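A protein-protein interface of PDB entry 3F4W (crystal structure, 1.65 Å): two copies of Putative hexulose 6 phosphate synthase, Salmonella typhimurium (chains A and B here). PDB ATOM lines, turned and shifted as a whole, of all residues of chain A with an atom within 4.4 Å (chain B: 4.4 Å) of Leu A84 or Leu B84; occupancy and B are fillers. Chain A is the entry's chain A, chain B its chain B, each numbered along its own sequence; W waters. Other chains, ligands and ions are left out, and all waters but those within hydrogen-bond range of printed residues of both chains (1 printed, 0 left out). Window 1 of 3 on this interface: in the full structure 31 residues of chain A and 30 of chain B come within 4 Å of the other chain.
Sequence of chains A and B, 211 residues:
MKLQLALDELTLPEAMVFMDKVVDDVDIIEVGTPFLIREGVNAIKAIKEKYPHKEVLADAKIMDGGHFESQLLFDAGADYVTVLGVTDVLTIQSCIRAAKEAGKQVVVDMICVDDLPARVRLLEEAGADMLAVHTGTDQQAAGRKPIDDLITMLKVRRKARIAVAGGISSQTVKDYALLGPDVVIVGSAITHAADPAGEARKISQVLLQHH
Of the printed residues of chain B, Lys A61 touches Met B63 (3.9 Å). Ile A62 touches none of the printed residues of chain B. Of the printed residues of chain B, Leu A84 touches Met B63 (3.99 Å) and Leu B84 (3.9 Å). Of the printed residues of chain B, Val A86 touches Met B63 (3.9 Å) and Val B86 (3.7 Å). Leu B84 touches just these residues of chain A: Met A63 (3.9 Å) and Leu A84 (3.9 Å). Of the printed residues of chain A, Ile B111 touches Met A63 (3.6 Å). The nearest printed residue of chain B that does not touch Leu A84 is Lys B61 (5.4 Å).
The backbone NH (N) of Leu A84 sits at hydrogen-bond distance from the backbone carbonyl oxygen (O) of Ile A62. O of Met A63 sits at hydrogen-bond distance from OG1 of Thr A87, 2.6 Å away. The backbone NH (N) of Ile A111 lies within hydrogen-bond range of the side-chain carboxylate (OD2) of Asp A109, 2.9 Å away. The backbone carbonyl oxygen (O) of Ile B62 lies within hydrogen-bond range of the backbone NH (N) of Leu B84 (2.9 Å). The backbone carbonyl oxygen of Met B63 is in hydrogen-bond range of the side-chain hydroxyl of Thr B87. OD2 of Asp B109 is in hydrogen-bond range of N of Ile B111 (2.9 Å).
Of the 12 printed residues of chain A, 5 touch a printed residue of chain B. Printed residues of chain A that touch a printed residue of chain B: Lys A61, Met A63, Leu A84, Val A86 and Ile A111. Hydrophobic or aromatic side chains of chain A that line the printed part of chain B: Met A63, Leu A84 and Val A86. Of the 12 printed residues of chain B, 4 touch a printed residue of chain A. Hydrophobic or aromatic side chains of chain B within 4 Å of the printed part of chain A: Met B63, Leu B84 and Val B86. Along chain B the printed residues that touch a printed residue of chain A span positions 63 to 111. Among the printed residues, 9 pairs touch across the chains.
Lys A61 touches Met B63, but with the chains exchanged Met A63 does not touch Lys B61 (4.04 Å). Met A63 touches Leu B84, and with the chains exchanged Leu A84 touches Met B63. Met A63 touches Ile B111, and with the chains exchanged Ile A111 touches Met B63. Leu B84 touches its own counterpart, Leu A84. Positions printed for both chains: 61, 62, 63, 83, 84, 85, 86, 87, 92, 108, 109 and 111.
CD of Lys A61 touches CB of Met B63 (3.9 Å). Leu B84 touches Met A63. CE of Met A63 touches CG2 of Val B86, at 3.9 Å. Met A63 touches Ile B111 (CE to O, 3.6 Å). CD2 of Leu A84 touches CG of Met B63, 3.99 Å away. CD2 of Leu B84 touches CD2 of Leu A84 (3.9 Å). CE of Met B63 touches CG2 of Val A86, at 3.9 Å. Val B86 touches Val A86 (CG2 to CG2, 3.7 Å). Ile A111 touches Met B63.
Water W1 bridges the backbone carbonyl oxygen of Lys B61 (2.7 Å) and the backbone carbonyl oxygen of Lys A61 (2.8 Å).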
ATOM      1  N   LYS A  61      28.448  14.992 -11.862  1.00  0.00           N
ATOM      2  CA  LYS A  61      28.178  14.305 -13.125  1.00  0.00           C
ATOM      3  C   LYS A  61      27.082  15.029 -13.901  1.00  0.00           C
ATOM      4  O   LYS A  61      26.094  14.424 -14.331  1.00  0.00           O
ATOM      5  CB  LYS A  61      27.781  12.844 -12.885  1.00  0.00           C
ATOM      6  CG  LYS A  61      28.943  11.920 -12.549  1.00  0.00           C
ATOM      7  CD  LYS A  61      28.477  10.472 -12.490  1.00  0.00           C
ATOM      8  CE  LYS A  61      29.613   9.530 -12.125  1.00  0.00           C
ATOM      9  NZ  LYS A  61      29.979   9.647 -10.690  1.00  0.00           N
ATOM     10  N   ILE A  62      27.274  16.330 -14.075  1.00  0.00           N
ATOM     11  CA  ILE A  62      26.305  17.188 -14.740  1.00  0.00           C
ATOM     12  C   ILE A  62      25.946  16.714 -16.150  1.00  0.00           C
ATOM     13  O   ILE A  62      26.818  16.354 -16.945  1.00  0.00           O
ATOM     14  CB  ILE A  62      26.818  18.638 -14.793  1.00  0.00           C
ATOM     15  CG1 ILE A  62      26.960  19.191 -13.373  1.00  0.00           C
ATOM     16  CG2 ILE A  62      25.876  19.513 -15.599  1.00  0.00           C
ATOM     17  CD1 ILE A  62      27.622  20.553 -13.310  1.00  0.00           C
ATOM     18  N   MET A  63      24.650  16.714 -16.448  1.00  0.00           N
ATOM     19  CA  MET A  63      24.151  16.261 -17.739  1.00  0.00           C
ATOM     20  C   MET A  63      23.363  17.376 -18.417  1.00  0.00           C
ATOM     21  O   MET A  63      23.153  17.358 -19.628  1.00  0.00           O
ATOM     22  CB  MET A  63      23.251  15.037 -17.555  1.00  0.00           C
ATOM     23  CG  MET A  63      22.800  14.383 -18.855  1.00  0.00           C
ATOM     24  SD  MET A  63      24.169  13.563 -19.694  1.00  0.00           S
ATOM     25  CE  MET A  63      23.419  13.052 -21.244  1.00  0.00           C
ATOM     26  N   VAL A  83      31.386  17.060 -15.223  1.00  0.00           N
ATOM     27  CA  VAL A  83      30.325  17.051 -16.217  1.00  0.00           C
ATOM     28  C   VAL A  83      30.532  15.798 -17.065  1.00  0.00           C
ATOM     29  O   VAL A  83      31.664  15.362 -17.262  1.00  0.00           O
ATOM     30  CB  VAL A  83      30.378  18.310 -17.111  1.00  0.00           C
ATOM     31  CG1 VAL A  83      31.671  18.336 -17.921  1.00  0.00           C
ATOM     32  CG2 VAL A  83      29.182  18.363 -18.038  1.00  0.00           C
ATOM     33  N   LEU A  84      29.446  15.208 -17.547  1.00  0.00           N
ATOM     34  CA  LEU A  84      29.530  13.976 -18.326  1.00  0.00           C
ATOM     35  C   LEU A  84      29.980  14.234 -19.758  1.00  0.00           C
ATOM     36  O   LEU A  84      29.423  15.087 -20.444  1.00  0.00           O
ATOM     37  CB  LEU A  84      28.175  13.266 -18.340  1.00  0.00           C
ATOM     38  CG  LEU A  84      27.871  12.149 -17.335  1.00  0.00           C
ATOM     39  CD1 LEU A  84      28.904  12.052 -16.232  1.00  0.00           C
ATOM     40  CD2 LEU A  84      26.461  12.330 -16.773  1.00  0.00           C
ATOM     41  N   GLY A  85      30.978  13.481 -20.208  1.00  0.00           N
ATOM     42  CA  GLY A  85      31.444  13.578 -21.579  1.00  0.00           C
ATOM     43  C   GLY A  85      30.369  13.204 -22.584  1.00  0.00           C
ATOM     44  O   GLY A  85      30.422  13.618 -23.742  1.00  0.00           O
ATOM     45  N   VAL A  86      29.384  12.424 -22.144  1.00  0.00           N
ATOM     46  CA  VAL A  86      28.319  11.984 -23.040  1.00  0.00           C
ATOM     47  C   VAL A  86      27.247  13.050 -23.243  1.00  0.00           C
ATOM     48  O   VAL A  86      26.362  12.886 -24.077  1.00  0.00           O
ATOM     49  CB  VAL A  86      27.650  10.670 -22.564  1.00  0.00           C
ATOM     50  CG1 VAL A  86      28.616   9.504 -22.701  1.00  0.00           C
ATOM     51  CG2 VAL A  86      27.157  10.799 -21.137  1.00  0.00           C
ATOM     52  N   THR A  87      27.325  14.142 -22.486  1.00  0.00           N
ATOM     53  CA  THR A  87      26.337  15.208 -22.620  1.00  0.00           C
ATOM     54  C   THR A  87      26.649  16.124 -23.801  1.00  0.00           C
ATOM     55  O   THR A  87      27.699  16.012 -24.432  1.00  0.00           O
ATOM     56  CB  THR A  87      26.200  16.052 -21.337  1.00  0.00           C
ATOM     57  OG1 THR A  87      24.966  16.781 -21.382  1.00  0.00           O
ATOM     58  CG2 THR A  87      27.358  17.032 -21.199  1.00  0.00           C
ATOM     59  N   ILE A  92      28.699  21.158 -21.677  1.00  0.00           N
ATOM     60  CA  ILE A  92      30.097  21.150 -21.273  1.00  0.00           C
ATOM     61  C   ILE A  92      30.647  22.569 -21.292  1.00  0.00           C
ATOM     62  O   ILE A  92      31.340  22.990 -20.367  1.00  0.00           O
ATOM     63  CB  ILE A  92      30.932  20.218 -22.158  1.00  0.00           C
ATOM     64  CG1 ILE A  92      30.616  18.764 -21.796  1.00  0.00           C
ATOM     65  CG2 ILE A  92      32.419  20.514 -21.994  1.00  0.00           C
ATOM     66  CD1 ILE A  92      31.256  17.748 -22.692  1.00  0.00           C
ATOM     67  N   VAL A 108      35.796  16.674 -17.207  1.00  0.00           N
ATOM     68  CA  VAL A 108      34.848  15.940 -18.036  1.00  0.00           C
ATOM     69  C   VAL A 108      35.007  14.447 -17.777  1.00  0.00           C
ATOM     70  O   VAL A 108      36.039  13.861 -18.099  1.00  0.00           O
ATOM     71  CB  VAL A 108      35.042  16.224 -19.535  1.00  0.00           C
ATOM     72  CG1 VAL A 108      33.933  15.557 -20.345  1.00  0.00           C
ATOM     73  CG2 VAL A 108      35.063  17.717 -19.798  1.00  0.00           C
ATOM     74  N   ASP A 109      33.989  13.844 -17.169  1.00  0.00           N
ATOM     75  CA  ASP A 109      34.013  12.420 -16.850  1.00  0.00           C
ATOM     76  C   ASP A 109      33.558  11.625 -18.061  1.00  0.00           C
ATOM     77  O   ASP A 109      32.413  11.741 -18.498  1.00  0.00           O
ATOM     78  CB  ASP A 109      33.113  12.132 -15.648  1.00  0.00           C
ATOM     79  CG  ASP A 109      33.157  10.675 -15.212  1.00  0.00           C
ATOM     80  OD1 ASP A 109      32.831  10.402 -14.041  1.00  0.00           O
ATOM     81  OD2 ASP A 109      33.510   9.801 -16.024  1.00  0.00           O
ATOM     82  N   ILE A 111      32.950   8.535 -18.549  1.00  0.00           N
ATOM     83  CA  ILE A 111      32.276   7.265 -18.313  1.00  0.00           C
ATOM     84  C   ILE A 111      31.241   6.977 -19.408  1.00  0.00           C
ATOM     85  O   ILE A 111      30.478   7.859 -19.802  1.00  0.00           O
ATOM     86  CB  ILE A 111      31.628   7.216 -16.908  1.00  0.00           C
ATOM     87  CG1 ILE A 111      30.962   5.858 -16.665  1.00  0.00           C
ATOM     88  CG2 ILE A 111      30.627   8.354 -16.726  1.00  0.00           C
ATOM     89  CD1 ILE A 111      30.298   5.750 -15.308  1.00  0.00           C
ATOM     90  N   LYS B  61      19.052  11.755 -12.514  1.00  0.00           N
ATOM     91  CA  LYS B  61      19.819  11.501 -13.734  1.00  0.00           C
ATOM     92  C   LYS B  61      21.012  10.595 -13.428  1.00  0.00           C
ATOM     93  O   LYS B  61      22.156  10.900 -13.768  1.00  0.00           O
ATOM     94  CB  LYS B  61      20.278  12.812 -14.383  1.00  0.00           C
ATOM     95  CG  LYS B  61      19.152  13.616 -15.026  1.00  0.00           C
ATOM     96  CD  LYS B  61      19.675  14.896 -15.672  1.00  0.00           C
ATOM     97  CE  LYS B  61      18.616  15.996 -15.676  1.00  0.00           C
ATOM     98  NZ  LYS B  61      17.647  15.843 -16.780  1.00  0.00           N
ATOM     99  N   ILE B  62      20.718   9.477 -12.777  1.00  0.00           N
ATOM    100  CA  ILE B  62      21.727   8.508 -12.371  1.00  0.00           C
ATOM    101  C   ILE B  62      22.590   8.018 -13.533  1.00  0.00           C
ATOM    102  O   ILE B  62      22.087   7.711 -14.616  1.00  0.00           O
ATOM    103  CB  ILE B  62      21.059   7.318 -11.664  1.00  0.00           C
ATOM    104  CG1 ILE B  62      20.452   7.785 -10.338  1.00  0.00           C
ATOM    105  CG2 ILE B  62      22.056   6.196 -11.434  1.00  0.00           C
ATOM    106  CD1 ILE B  62      19.638   6.729  -9.637  1.00  0.00           C
ATOM    107  N   MET B  63      23.898   7.954 -13.299  1.00  0.00           N
ATOM    108  CA  MET B  63      24.853   7.549 -14.326  1.00  0.00           C
ATOM    109  C   MET B  63      25.687   6.375 -13.831  1.00  0.00           C
ATOM    110  O   MET B  63      26.286   5.650 -14.622  1.00  0.00           O
ATOM    111  CB  MET B  63      25.776   8.716 -14.682  1.00  0.00           C
ATOM    112  CG  MET B  63      26.699   8.455 -15.863  1.00  0.00           C
ATOM    113  SD  MET B  63      25.776   8.310 -17.407  1.00  0.00           S
ATOM    114  CE  MET B  63      27.048   7.808 -18.566  1.00  0.00           C
ATOM    115  N   VAL B  83      17.142   7.670 -14.457  1.00  0.00           N
ATOM    116  CA  VAL B  83      18.474   7.189 -14.807  1.00  0.00           C
ATOM    117  C   VAL B  83      18.737   7.576 -16.261  1.00  0.00           C
ATOM    118  O   VAL B  83      17.815   7.601 -17.073  1.00  0.00           O
ATOM    119  CB  VAL B  83      18.582   5.654 -14.661  1.00  0.00           C
ATOM    120  CG1 VAL B  83      17.622   4.955 -15.617  1.00  0.00           C
ATOM    121  CG2 VAL B  83      20.004   5.188 -14.912  1.00  0.00           C
ATOM    122  N   LEU B  84      19.986   7.885 -16.581  1.00  0.00           N
ATOM    123  CA  LEU B  84      20.365   8.291 -17.933  1.00  0.00           C
ATOM    124  C   LEU B  84      20.342   7.135 -18.925  1.00  0.00           C
ATOM    125  O   LEU B  84      20.963   6.102 -18.690  1.00  0.00           O
ATOM    126  CB  LEU B  84      21.758   8.918 -17.914  1.00  0.00           C
ATOM    127  CG  LEU B  84      21.872  10.439 -18.017  1.00  0.00           C
ATOM    128  CD1 LEU B  84      20.528  11.125 -17.901  1.00  0.00           C
ATOM    129  CD2 LEU B  84      22.859  10.965 -16.987  1.00  0.00           C
ATOM    130  N   GLY B  85      19.636   7.321 -20.038  1.00  0.00           N
ATOM    131  CA  GLY B  85      19.599   6.331 -21.101  1.00  0.00           C
ATOM    132  C   GLY B  85      20.970   6.056 -21.697  1.00  0.00           C
ATOM    133  O   GLY B  85      21.204   4.982 -22.252  1.00  0.00           O
ATOM    134  N   VAL B  86      21.881   7.022 -21.579  1.00  0.00           N
ATOM    135  CA  VAL B  86      23.230   6.874 -22.130  1.00  0.00           C
ATOM    136  C   VAL B  86      24.161   6.069 -21.226  1.00  0.00           C
ATOM    137  O   VAL B  86      25.278   5.745 -21.620  1.00  0.00           O
ATOM    138  CB  VAL B  86      23.906   8.242 -22.449  1.00  0.00           C
ATOM    139  CG1 VAL B  86      23.231   8.919 -23.631  1.00  0.00           C
ATOM    140  CG2 VAL B  86      23.903   9.148 -21.233  1.00  0.00           C
ATOM    141  N   THR B  87      23.712   5.749 -20.016  1.00  0.00           N
ATOM    142  CA  THR B  87      24.550   4.986 -19.096  1.00  0.00           C
ATOM    143  C   THR B  87      24.554   3.501 -19.443  1.00  0.00           C
ATOM    144  O   THR B  87      23.797   3.051 -20.301  1.00  0.00           O
ATOM    145  CB  THR B  87      24.108   5.155 -17.631  1.00  0.00           C
ATOM    146  OG1 THR B  87      25.175   4.744 -16.766  1.00  0.00           O
ATOM    147  CG2 THR B  87      22.878   4.309 -17.338  1.00  0.00           C
ATOM    148  N   ILE B  92      21.315   0.759 -15.476  1.00  0.00           N
ATOM    149  CA  ILE B  92      19.878   0.816 -15.685  1.00  0.00           C
ATOM    150  C   ILE B  92      19.197  -0.335 -14.950  1.00  0.00           C
ATOM    151  O   ILE B  92      18.215  -0.136 -14.234  1.00  0.00           O
ATOM    152  CB  ILE B  92      19.525   0.795 -17.182  1.00  0.00           C
ATOM    153  CG1 ILE B  92      20.067   2.058 -17.858  1.00  0.00           C
ATOM    154  CG2 ILE B  92      18.024   0.677 -17.380  1.00  0.00           C
ATOM    155  CD1 ILE B  92      19.254   2.519 -19.042  1.00  0.00           C
ATOM    156  N   VAL B 108      13.717   6.124 -17.533  1.00  0.00           N
ATOM    157  CA  VAL B 108      14.965   6.288 -18.267  1.00  0.00           C
ATOM    158  C   VAL B 108      14.913   7.575 -19.078  1.00  0.00           C
ATOM    159  O   VAL B 108      14.128   7.694 -20.018  1.00  0.00           O
ATOM    160  CB  VAL B 108      15.229   5.111 -19.216  1.00  0.00           C
ATOM    161  CG1 VAL B 108      16.580   5.288 -19.920  1.00  0.00           C
ATOM    162  CG2 VAL B 108      15.192   3.800 -18.457  1.00  0.00           C
ATOM    163  N   ASP B 109      15.742   8.540 -18.701  1.00  0.00           N
ATOM    164  CA  ASP B 109      15.797   9.815 -19.403  1.00  0.00           C
ATOM    165  C   ASP B 109      16.719   9.687 -20.606  1.00  0.00           C
ATOM    166  O   ASP B 109      17.916   9.446 -20.459  1.00  0.00           O
ATOM    167  CB  ASP B 109      16.284  10.911 -18.456  1.00  0.00           C
ATOM    168  CG  ASP B 109      16.282  12.284 -19.097  1.00  0.00           C
ATOM    169  OD1 ASP B 109      16.274  13.282 -18.352  1.00  0.00           O
ATOM    170  OD2 ASP B 109      16.290  12.374 -20.338  1.00  0.00           O
ATOM    171  N   ILE B 111      17.805  11.803 -22.735  1.00  0.00           N
ATOM    172  CA  ILE B 111      18.511  13.012 -23.149  1.00  0.00           C
ATOM    173  C   ILE B 111      19.883  12.679 -23.746  1.00  0.00           C
ATOM    174  O   ILE B 111      20.639  11.884 -23.187  1.00  0.00           O
ATOM    175  CB  ILE B 111      18.642  14.020 -21.975  1.00  0.00           C
ATOM    176  CG1 ILE B 111      19.274  15.331 -22.450  1.00  0.00           C
ATOM    177  CG2 ILE B 111      19.436  13.416 -20.813  1.00  0.00           C
ATOM    178  CD1 ILE B 111      19.470  16.343 -21.339  1.00  0.00           C
HETATM  179  O   HOH W   1      24.480  12.315 -13.517  1.00  0.00           O
